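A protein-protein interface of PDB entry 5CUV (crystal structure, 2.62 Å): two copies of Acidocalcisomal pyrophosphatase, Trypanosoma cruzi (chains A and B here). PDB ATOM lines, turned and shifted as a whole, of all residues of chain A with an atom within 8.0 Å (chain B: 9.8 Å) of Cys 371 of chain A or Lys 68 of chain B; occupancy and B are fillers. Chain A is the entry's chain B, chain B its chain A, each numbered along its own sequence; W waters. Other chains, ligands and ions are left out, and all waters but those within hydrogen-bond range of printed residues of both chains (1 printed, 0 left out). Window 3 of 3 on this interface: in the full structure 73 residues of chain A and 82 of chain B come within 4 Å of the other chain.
O of Arg 235 of chain A lies within hydrogen-bond range of N of Tyr 261 of chain A (2.9 Å). The guanidinium group of Arg 235 of chain A lies within salt-bridge range of the side-chain carboxylate of Asp 265 of chain A (2.8 Å).
No position is printed for both chains. Of the 10 pairs that touch across the chains among the printed residues, none has its exchanged pair printed and touching as well.
Of the 16 printed residues of chain A, 4 touch a printed residue of chain B. Hydrophobic or aromatic side chains of chain A within 4 Å of the printed part of chain B: Phe 260. Hydrophobic or aromatic side chains of chain B within 4 Å of the printed part of chain A: Tyr 66. Among the printed residues, 10 pairs touch across the chains. Among the printed residues, no Asp or Glu carboxylate lies within 4 Å of a Lys or Arg side-chain nitrogen of the other chain.
Water W1 lies within hydrogen-bond range of O of Asp 69 of chain B, NZ of Lys 262 of chain A and O of Val 64 of chain B.
The backbone carbonyl oxygen (O) of Gly 67 of chain B sits at hydrogen-bond distance from the side-chain amino group (NZ) of Lys 262 of chain A (3.3 Å). O of Ala 65 of chain B sits at hydrogen-bond distance from NZ of Lys 262 of chain A, at 3.4 Å. The side-chain amino group (NZ) of Lys 262 of chain A sits at hydrogen-bond distance from the backbone carbonyl oxygen (O) of Val 64 of chain B, at 2.5 Å. NZ of Lys 68 of chain B lies within hydrogen-bond range of O of Lys 262 of chain A, 2.4 Å away.
Among the printed residues, pairs that only touch across the chains: Cys 371 of chain A with Lys 68 of chain B (3.7 Å), Phe 260 of chain A with Val 64 of chain B (3.7 Å), Phe 260 of chain A with Ala 65 of chain B (3.8 Å), Arg 235 of chain A with Ala 65 of chain B (3.9 Å), Lys 262 of chain A with Glu 70 of chain B (3.9 Å) and Arg 235 of chain A with Tyr 66 of chain B (3.98 Å).
Of the printed residues of chain B, Phe 260 of chain A touches Val 64 (3.7 Å) and Ala 65 (3.8 Å). Printed residues of chain B within 4 Å of Lys 262 of chain A: Val 64, Ala 65, Gly 67, Lys 68 and Glu 70. Tyr 368 of chain A touches none of the printed residues of chain B. Cys 371 of chain A touches just one residue of chain B: Lys 68. Of the printed residues of chain A, Val 64 of chain B touches Phe 260 and Lys 262. Of the printed residues of chain A, Tyr 66 of chain B touches Arg 235 (3.98 Å). Of the printed residues of chain A, Glu 70 of chain B touches Lys 262. The nearest residue of chain A that does not touch Lys 68 of chain B is Arg 235 of chain A (4.2 Å). The nearest printed residue of chain A that does not touch Ala 65 of chain B is Tyr 261 of chain A (5.0 Å).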
ATOM      1  N   ARG A 235       7.904   4.637 -32.161  1.00  0.00           N
ATOM      2  CA  ARG A 235       7.094   4.947 -31.014  1.00  0.00           C
ATOM      3  C   ARG A 235       6.037   3.920 -30.644  1.00  0.00           C
ATOM      4  O   ARG A 235       5.257   4.189 -29.765  1.00  0.00           O
ATOM      5  CB  ARG A 235       6.443   6.339 -31.195  1.00  0.00           C
ATOM      6  CG  ARG A 235       5.235   6.403 -32.125  1.00  0.00           C
ATOM      7  CD  ARG A 235       4.733   7.820 -32.274  1.00  0.00           C
ATOM      8  NE  ARG A 235       5.803   8.721 -32.721  1.00  0.00           N
ATOM      9  CZ  ARG A 235       5.689  10.041 -32.763  1.00  0.00           C
ATOM     10  NH1 ARG A 235       4.581  10.642 -32.406  1.00  0.00           N
ATOM     11  NH2 ARG A 235       6.694  10.754 -33.147  1.00  0.00           N
ATOM     12  N   PHE A 260       0.814   3.497 -28.762  1.00  0.00           N
ATOM     13  CA  PHE A 260       2.002   4.273 -29.111  1.00  0.00           C
ATOM     14  C   PHE A 260       2.337   5.446 -28.161  1.00  0.00           C
ATOM     15  O   PHE A 260       1.439   6.221 -27.751  1.00  0.00           O
ATOM     16  CB  PHE A 260       1.827   4.881 -30.507  1.00  0.00           C
ATOM     17  CG  PHE A 260       1.457   3.881 -31.566  1.00  0.00           C
ATOM     18  CD1 PHE A 260       0.137   3.468 -31.727  1.00  0.00           C
ATOM     19  CD2 PHE A 260       2.425   3.350 -32.405  1.00  0.00           C
ATOM     20  CE1 PHE A 260      -0.205   2.539 -32.714  1.00  0.00           C
ATOM     21  CE2 PHE A 260       2.101   2.424 -33.393  1.00  0.00           C
ATOM     22  CZ  PHE A 260       0.780   2.013 -33.550  1.00  0.00           C
ATOM     23  N   TYR A 261       3.632   5.598 -27.839  1.00  0.00           N
ATOM     24  CA  TYR A 261       4.086   6.781 -27.057  1.00  0.00           C
ATOM     25  C   TYR A 261       3.638   7.997 -27.833  1.00  0.00           C
ATOM     26  O   TYR A 261       4.004   8.091 -28.994  1.00  0.00           O
ATOM     27  CB  TYR A 261       5.588   6.902 -26.990  1.00  0.00           C
ATOM     28  CG  TYR A 261       6.181   5.962 -26.030  1.00  0.00           C
ATOM     29  CD1 TYR A 261       5.926   6.106 -24.675  1.00  0.00           C
ATOM     30  CD2 TYR A 261       6.938   4.862 -26.468  1.00  0.00           C
ATOM     31  CE1 TYR A 261       6.390   5.182 -23.765  1.00  0.00           C
ATOM     32  CE2 TYR A 261       7.426   3.910 -25.545  1.00  0.00           C
ATOM     33  CZ  TYR A 261       7.134   4.089 -24.199  1.00  0.00           C
ATOM     34  OH  TYR A 261       7.521   3.179 -23.268  1.00  0.00           O
ATOM     35  N   LYS A 262       2.893   8.909 -27.208  1.00  0.00           N
ATOM     36  CA  LYS A 262       2.405  10.118 -27.896  1.00  0.00           C
ATOM     37  C   LYS A 262       3.374  11.304 -27.811  1.00  0.00           C
ATOM     38  O   LYS A 262       3.257  12.313 -28.520  1.00  0.00           O
ATOM     39  CB  LYS A 262       1.043  10.572 -27.319  1.00  0.00           C
ATOM     40  CG  LYS A 262      -0.078   9.580 -27.435  1.00  0.00           C
ATOM     41  CD  LYS A 262      -0.179   9.158 -28.835  1.00  0.00           C
ATOM     42  CE  LYS A 262      -1.278   8.134 -29.017  1.00  0.00           C
ATOM     43  NZ  LYS A 262      -1.349   7.726 -30.459  1.00  0.00           N
ATOM     44  N   HIS A 263       4.332  11.179 -26.927  1.00  0.00           N
ATOM     45  CA  HIS A 263       5.270  12.241 -26.735  1.00  0.00           C
ATOM     46  C   HIS A 263       6.211  12.410 -27.910  1.00  0.00           C
ATOM     47  O   HIS A 263       6.646  13.514 -28.220  1.00  0.00           O
ATOM     48  CB  HIS A 263       6.087  11.954 -25.490  1.00  0.00           C
ATOM     49  CG  HIS A 263       7.231  12.898 -25.294  1.00  0.00           C
ATOM     50  ND1 HIS A 263       7.054  14.222 -24.944  1.00  0.00           N
ATOM     51  CD2 HIS A 263       8.569  12.706 -25.376  1.00  0.00           C
ATOM     52  CE1 HIS A 263       8.233  14.802 -24.809  1.00  0.00           C
ATOM     53  NE2 HIS A 263       9.170  13.903 -25.067  1.00  0.00           N
ATOM     54  N   GLY A 264       6.550  11.305 -28.547  1.00  0.00           N
ATOM     55  CA  GLY A 264       7.490  11.384 -29.635  1.00  0.00           C
ATOM     56  C   GLY A 264       8.143  10.032 -29.728  1.00  0.00           C
ATOM     57  O   GLY A 264       7.867   9.148 -28.944  1.00  0.00           O
ATOM     58  N   ASP A 265       9.022   9.874 -30.679  1.00  0.00           N
ATOM     59  CA  ASP A 265       9.709   8.623 -30.864  1.00  0.00           C
ATOM     60  C   ASP A 265      10.747   8.482 -29.828  1.00  0.00           C
ATOM     61  O   ASP A 265      11.187   9.470 -29.276  1.00  0.00           O
ATOM     62  CB  ASP A 265      10.328   8.606 -32.265  1.00  0.00           C
ATOM     63  CG  ASP A 265       9.266   8.647 -33.328  1.00  0.00           C
ATOM     64  OD1 ASP A 265       8.405   7.746 -33.279  1.00  0.00           O
ATOM     65  OD2 ASP A 265       9.245   9.573 -34.157  1.00  0.00           O
ATOM     66  N   VAL A 367       9.404  13.992 -19.005  1.00  0.00           N
ATOM     67  CA  VAL A 367       8.171  14.526 -19.512  1.00  0.00           C
ATOM     68  C   VAL A 367       7.335  13.746 -20.474  1.00  0.00           C
ATOM     69  O   VAL A 367       6.325  14.263 -20.949  1.00  0.00           O
ATOM     70  CB  VAL A 367       8.430  15.947 -20.121  1.00  0.00           C
ATOM     71  CG1 VAL A 367       9.393  16.704 -19.220  1.00  0.00           C
ATOM     72  CG2 VAL A 367       9.013  15.860 -21.543  1.00  0.00           C
ATOM     73  N   TYR A 368       7.674  12.499 -20.733  1.00  0.00           N
ATOM     74  CA  TYR A 368       6.901  11.753 -21.709  1.00  0.00           C
ATOM     75  C   TYR A 368       5.416  11.542 -21.367  1.00  0.00           C
ATOM     76  O   TYR A 368       4.656  10.978 -22.210  1.00  0.00           O
ATOM     77  CB  TYR A 368       7.593  10.419 -22.024  1.00  0.00           C
ATOM     78  CG  TYR A 368       7.389   9.329 -21.024  1.00  0.00           C
ATOM     79  CD1 TYR A 368       6.308   8.498 -21.112  1.00  0.00           C
ATOM     80  CD2 TYR A 368       8.314   9.109 -19.992  1.00  0.00           C
ATOM     81  CE1 TYR A 368       6.141   7.456 -20.207  1.00  0.00           C
ATOM     82  CE2 TYR A 368       8.157   8.065 -19.067  1.00  0.00           C
ATOM     83  CZ  TYR A 368       7.061   7.238 -19.178  1.00  0.00           C
ATOM     84  OH  TYR A 368       6.821   6.221 -18.252  1.00  0.00           O
ATOM     85  N   LYS A 369       4.985  11.976 -20.163  1.00  0.00           N
ATOM     86  CA  LYS A 369       3.555  11.871 -19.800  1.00  0.00           C
ATOM     87  C   LYS A 369       2.729  13.185 -19.817  1.00  0.00           C
ATOM     88  O   LYS A 369       1.487  13.143 -19.749  1.00  0.00           O
ATOM     89  CB  LYS A 369       3.378  11.237 -18.446  1.00  0.00           C
ATOM     90  CG  LYS A 369       4.010   9.883 -18.285  1.00  0.00           C
ATOM     91  CD  LYS A 369       3.710   9.422 -16.901  1.00  0.00           C
ATOM     92  CE  LYS A 369       4.455   8.198 -16.518  1.00  0.00           C
ATOM     93  NZ  LYS A 369       4.591   8.131 -15.003  1.00  0.00           N
ATOM     94  N   ILE A 370       3.383  14.343 -19.920  1.00  0.00           N
ATOM     95  CA  ILE A 370       2.651  15.623 -19.894  1.00  0.00           C
ATOM     96  C   ILE A 370       1.646  15.758 -21.050  1.00  0.00           C
ATOM     97  O   ILE A 370       0.550  16.224 -20.875  1.00  0.00           O
ATOM     98  CB  ILE A 370       3.693  16.811 -19.798  1.00  0.00           C
ATOM     99  CG1 ILE A 370       4.518  16.579 -18.529  1.00  0.00           C
ATOM    100  CG2 ILE A 370       3.032  18.190 -19.797  1.00  0.00           C
ATOM    101  CD1 ILE A 370       5.360  17.718 -18.089  1.00  0.00           C
ATOM    102  N   CYS A 371       2.011  15.297 -22.228  1.00  0.00           N
ATOM    103  CA  CYS A 371       1.124  15.344 -23.400  1.00  0.00           C
ATOM    104  C   CYS A 371      -0.242  14.631 -23.199  1.00  0.00           C
ATOM    105  O   CYS A 371      -1.253  15.043 -23.774  1.00  0.00           O
ATOM    106  CB  CYS A 371       1.862  14.716 -24.603  1.00  0.00           C
ATOM    107  SG  CYS A 371       0.910  14.454 -26.138  1.00  0.00           S
ATOM    108  N   GLN A 372      -0.256  13.555 -22.416  1.00  0.00           N
ATOM    109  CA  GLN A 372      -1.476  12.801 -22.188  1.00  0.00           C
ATOM    110  C   GLN A 372      -2.237  13.281 -20.921  1.00  0.00           C
ATOM    111  O   GLN A 372      -3.221  12.684 -20.501  1.00  0.00           O
ATOM    112  CB  GLN A 372      -1.142  11.287 -22.079  1.00  0.00           C
ATOM    113  CG  GLN A 372      -0.759  10.550 -23.409  1.00  0.00           C
ATOM    114  CD  GLN A 372       0.073   9.223 -23.182  1.00  0.00           C
ATOM    115  OE1 GLN A 372       0.845   8.770 -24.081  1.00  0.00           O
ATOM    116  NE2 GLN A 372      -0.086   8.611 -21.980  1.00  0.00           N
ATOM    117  N   GLY A 373      -1.792  14.361 -20.307  1.00  0.00           N
ATOM    118  CA  GLY A 373      -2.472  14.822 -19.107  1.00  0.00           C
ATOM    119  C   GLY A 373      -1.673  14.629 -17.821  1.00  0.00           C
ATOM    120  O   GLY A 373      -1.907  15.303 -16.803  1.00  0.00           O
ATOM    121  N   GLY A 374      -0.694  13.734 -17.864  1.00  0.00           N
ATOM    122  CA  GLY A 374       0.073  13.464 -16.671  1.00  0.00           C
ATOM    123  C   GLY A 374       0.914  14.654 -16.298  1.00  0.00           C
ATOM    124  O   GLY A 374       0.704  15.744 -16.833  1.00  0.00           O
ATOM    125  N   VAL A 375       1.855  14.419 -15.390  1.00  0.00           N
ATOM    126  CA  VAL A 375       2.780  15.416 -14.920  1.00  0.00           C
ATOM    127  C   VAL A 375       4.186  14.857 -15.012  1.00  0.00           C
ATOM    128  O   VAL A 375       4.373  13.706 -15.268  1.00  0.00           O
ATOM    129  CB  VAL A 375       2.523  15.791 -13.458  1.00  0.00           C
ATOM    130  CG1 VAL A 375       1.230  16.539 -13.359  1.00  0.00           C
ATOM    131  CG2 VAL A 375       2.535  14.557 -12.598  1.00  0.00           C
ATOM    132  N   ARG B  56     -11.229  13.631 -41.336  1.00  0.00           N
ATOM    133  CA  ARG B  56      -9.915  14.275 -41.396  1.00  0.00           C
ATOM    134  C   ARG B  56      -9.073  14.037 -42.633  1.00  0.00           C
ATOM    135  O   ARG B  56      -8.246  14.874 -42.946  1.00  0.00           O
ATOM    136  CB  ARG B  56      -9.080  13.916 -40.163  1.00  0.00           C
ATOM    137  CG  ARG B  56      -9.552  14.623 -38.921  1.00  0.00           C
ATOM    138  CD  ARG B  56      -8.476  14.696 -37.908  1.00  0.00           C
ATOM    139  NE  ARG B  56      -7.269  15.252 -38.510  1.00  0.00           N
ATOM    140  CZ  ARG B  56      -6.058  15.096 -37.997  1.00  0.00           C
ATOM    141  NH1 ARG B  56      -5.912  14.403 -36.877  1.00  0.00           N
ATOM    142  NH2 ARG B  56      -5.003  15.612 -38.602  1.00  0.00           N
ATOM    143  N   VAL B  58      -7.165  11.407 -43.003  1.00  0.00           N
ATOM    144  CA  VAL B  58      -6.057  10.746 -42.375  1.00  0.00           C
ATOM    145  C   VAL B  58      -6.508   9.283 -42.204  1.00  0.00           C
ATOM    146  O   VAL B  58      -7.653   9.030 -41.882  1.00  0.00           O
ATOM    147  CB  VAL B  58      -5.851  11.445 -41.029  1.00  0.00           C
ATOM    148  CG1 VAL B  58      -5.565  10.460 -39.926  1.00  0.00           C
ATOM    149  CG2 VAL B  58      -4.808  12.487 -41.172  1.00  0.00           C
ATOM    150  N   PHE B  61      -4.654   4.234 -39.200  1.00  0.00           N
ATOM    151  CA  PHE B  61      -3.330   3.939 -38.677  1.00  0.00           C
ATOM    152  C   PHE B  61      -2.692   5.203 -38.222  1.00  0.00           C
ATOM    153  O   PHE B  61      -2.182   5.275 -37.129  1.00  0.00           O
ATOM    154  CB  PHE B  61      -2.404   3.297 -39.699  1.00  0.00           C
ATOM    155  CG  PHE B  61      -1.114   2.895 -39.117  1.00  0.00           C
ATOM    156  CD1 PHE B  61      -1.027   1.739 -38.363  1.00  0.00           C
ATOM    157  CD2 PHE B  61      -0.011   3.772 -39.153  1.00  0.00           C
ATOM    158  CE1 PHE B  61       0.118   1.436 -37.626  1.00  0.00           C
ATOM    159  CE2 PHE B  61       1.181   3.500 -38.399  1.00  0.00           C
ATOM    160  CZ  PHE B  61       1.232   2.320 -37.629  1.00  0.00           C
ATOM    161  N   ASP B  62      -2.737   6.196 -39.083  1.00  0.00           N
ATOM    162  CA  ASP B  62      -2.143   7.494 -38.814  1.00  0.00           C
ATOM    163  C   ASP B  62      -2.732   8.236 -37.632  1.00  0.00           C
ATOM    164  O   ASP B  62      -2.012   8.950 -36.912  1.00  0.00           O
ATOM    165  CB  ASP B  62      -2.246   8.380 -40.058  1.00  0.00           C
ATOM    166  CG  ASP B  62      -1.155   8.094 -41.071  1.00  0.00           C
ATOM    167  OD1 ASP B  62      -0.306   7.209 -40.821  1.00  0.00           O
ATOM    168  OD2 ASP B  62      -1.147   8.755 -42.130  1.00  0.00           O
ATOM    169  N   LEU B  63      -4.048   8.087 -37.472  1.00  0.00           N
ATOM    170  CA  LEU B  63      -4.783   8.728 -36.415  1.00  0.00           C
ATOM    171  C   LEU B  63      -4.443   8.032 -35.109  1.00  0.00           C
ATOM    172  O   LEU B  63      -4.159   8.710 -34.118  1.00  0.00           O
ATOM    173  CB  LEU B  63      -6.283   8.693 -36.713  1.00  0.00           C
ATOM    174  CG  LEU B  63      -7.234   9.094 -35.556  1.00  0.00           C
ATOM    175  CD1 LEU B  63      -6.804  10.445 -34.999  1.00  0.00           C
ATOM    176  CD2 LEU B  63      -8.699   9.154 -36.009  1.00  0.00           C
ATOM    177  N   VAL B  64      -4.456   6.702 -35.064  1.00  0.00           N
ATOM    178  CA  VAL B  64      -4.091   6.078 -33.795  1.00  0.00           C
ATOM    179  C   VAL B  64      -2.565   6.199 -33.466  1.00  0.00           C
ATOM    180  O   VAL B  64      -2.177   6.328 -32.312  1.00  0.00           O
ATOM    181  CB  VAL B  64      -4.483   4.571 -33.740  1.00  0.00           C
ATOM    182  CG1 VAL B  64      -3.735   3.775 -34.829  1.00  0.00           C
ATOM    183  CG2 VAL B  64      -4.140   4.012 -32.378  1.00  0.00           C
ATOM    184  N   ALA B  65      -1.715   6.151 -34.484  1.00  0.00           N
ATOM    185  CA  ALA B  65      -0.267   6.235 -34.296  1.00  0.00           C
ATOM    186  C   ALA B  65       0.239   7.613 -33.904  1.00  0.00           C
ATOM    187  O   ALA B  65       0.936   7.752 -32.923  1.00  0.00           O
ATOM    188  CB  ALA B  65       0.462   5.770 -35.577  1.00  0.00           C
ATOM    189  N   TYR B  66      -0.152   8.621 -34.660  1.00  0.00           N
ATOM    190  CA  TYR B  66       0.317   9.968 -34.432  1.00  0.00           C
ATOM    191  C   TYR B  66      -0.649  11.034 -33.931  1.00  0.00           C
ATOM    192  O   TYR B  66      -0.218  12.131 -33.627  1.00  0.00           O
ATOM    193  CB  TYR B  66       0.946  10.469 -35.719  1.00  0.00           C
ATOM    194  CG  TYR B  66       1.794   9.413 -36.323  1.00  0.00           C
ATOM    195  CD1 TYR B  66       2.932   8.920 -35.647  1.00  0.00           C
ATOM    196  CD2 TYR B  66       1.467   8.869 -37.577  1.00  0.00           C
ATOM    197  CE1 TYR B  66       3.742   7.891 -36.219  1.00  0.00           C
ATOM    198  CE2 TYR B  66       2.255   7.872 -38.149  1.00  0.00           C
ATOM    199  CZ  TYR B  66       3.389   7.393 -37.469  1.00  0.00           C
ATOM    200  OH  TYR B  66       4.156   6.483 -38.097  1.00  0.00           O
ATOM    201  N   GLY B  67      -1.946  10.738 -33.893  1.00  0.00           N
ATOM    202  CA  GLY B  67      -2.900  11.701 -33.396  1.00  0.00           C
ATOM    203  C   GLY B  67      -2.653  11.746 -31.915  1.00  0.00           C
ATOM    204  O   GLY B  67      -2.487  10.679 -31.308  1.00  0.00           O
ATOM    205  N   LYS B  68      -2.633  12.950 -31.335  1.00  0.00           N
ATOM    206  CA  LYS B  68      -2.379  13.132 -29.904  1.00  0.00           C
ATOM    207  C   LYS B  68      -3.459  12.615 -29.004  1.00  0.00           C
ATOM    208  O   LYS B  68      -3.195  12.322 -27.841  1.00  0.00           O
ATOM    209  CB  LYS B  68      -2.140  14.601 -29.557  1.00  0.00           C
ATOM    210  CG  LYS B  68      -0.832  15.148 -30.165  1.00  0.00           C
ATOM    211  CD  LYS B  68       0.367  14.286 -29.776  1.00  0.00           C
ATOM    212  CE  LYS B  68       1.590  14.750 -30.496  1.00  0.00           C
ATOM    213  NZ  LYS B  68       2.680  13.757 -30.356  1.00  0.00           N
ATOM    214  N   ASP B  69      -4.685  12.493 -29.496  1.00  0.00           N
ATOM    215  CA  ASP B  69      -5.723  11.990 -28.597  1.00  0.00           C
ATOM    216  C   ASP B  69      -5.907  10.527 -28.644  1.00  0.00           C
ATOM    217  O   ASP B  69      -5.540   9.867 -29.596  1.00  0.00           O
ATOM    218  CB  ASP B  69      -7.050  12.657 -28.856  1.00  0.00           C
ATOM    219  CG  ASP B  69      -7.060  14.070 -28.343  1.00  0.00           C
ATOM    220  OD1 ASP B  69      -6.528  14.286 -27.224  1.00  0.00           O
ATOM    221  OD2 ASP B  69      -7.589  14.958 -29.041  1.00  0.00           O
ATOM    222  N   GLU B  70      -6.463  10.016 -27.572  1.00  0.00           N
ATOM    223  CA  GLU B  70      -6.736   8.613 -27.458  1.00  0.00           C
ATOM    224  C   GLU B  70      -8.068   8.373 -28.120  1.00  0.00           C
ATOM    225  O   GLU B  70      -8.833   9.311 -28.377  1.00  0.00           O
ATOM    226  CB  GLU B  70      -6.820   8.271 -26.002  1.00  0.00           C
ATOM    227  CG  GLU B  70      -5.511   8.566 -25.334  1.00  0.00           C
ATOM    228  CD  GLU B  70      -4.643   7.342 -25.247  1.00  0.00           C
ATOM    229  OE1 GLU B  70      -4.985   6.473 -24.395  1.00  0.00           O
ATOM    230  OE2 GLU B  70      -3.651   7.254 -26.030  1.00  0.00           O
ATOM    231  N   PHE B  71      -8.339   7.113 -28.419  1.00  0.00           N
ATOM    232  CA  PHE B  71      -9.592   6.778 -29.027  1.00  0.00           C
ATOM    233  C   PHE B  71     -10.638   6.920 -27.953  1.00  0.00           C
ATOM    234  O   PHE B  71     -10.371   6.668 -26.779  1.00  0.00           O
ATOM    235  CB  PHE B  71      -9.545   5.351 -29.573  1.00  0.00           C
ATOM    236  CG  PHE B  71      -9.087   5.273 -30.989  1.00  0.00           C
ATOM    237  CD1 PHE B  71      -8.258   6.288 -31.532  1.00  0.00           C
ATOM    238  CD2 PHE B  71      -9.460   4.196 -31.794  1.00  0.00           C
ATOM    239  CE1 PHE B  71      -7.806   6.221 -32.881  1.00  0.00           C
ATOM    240  CE2 PHE B  71      -9.020   4.110 -33.132  1.00  0.00           C
ATOM    241  CZ  PHE B  71      -8.191   5.122 -33.675  1.00  0.00           C
HETATM  242  O   HOH W   1      -4.202   7.409 -30.081  1.00  0.00           O
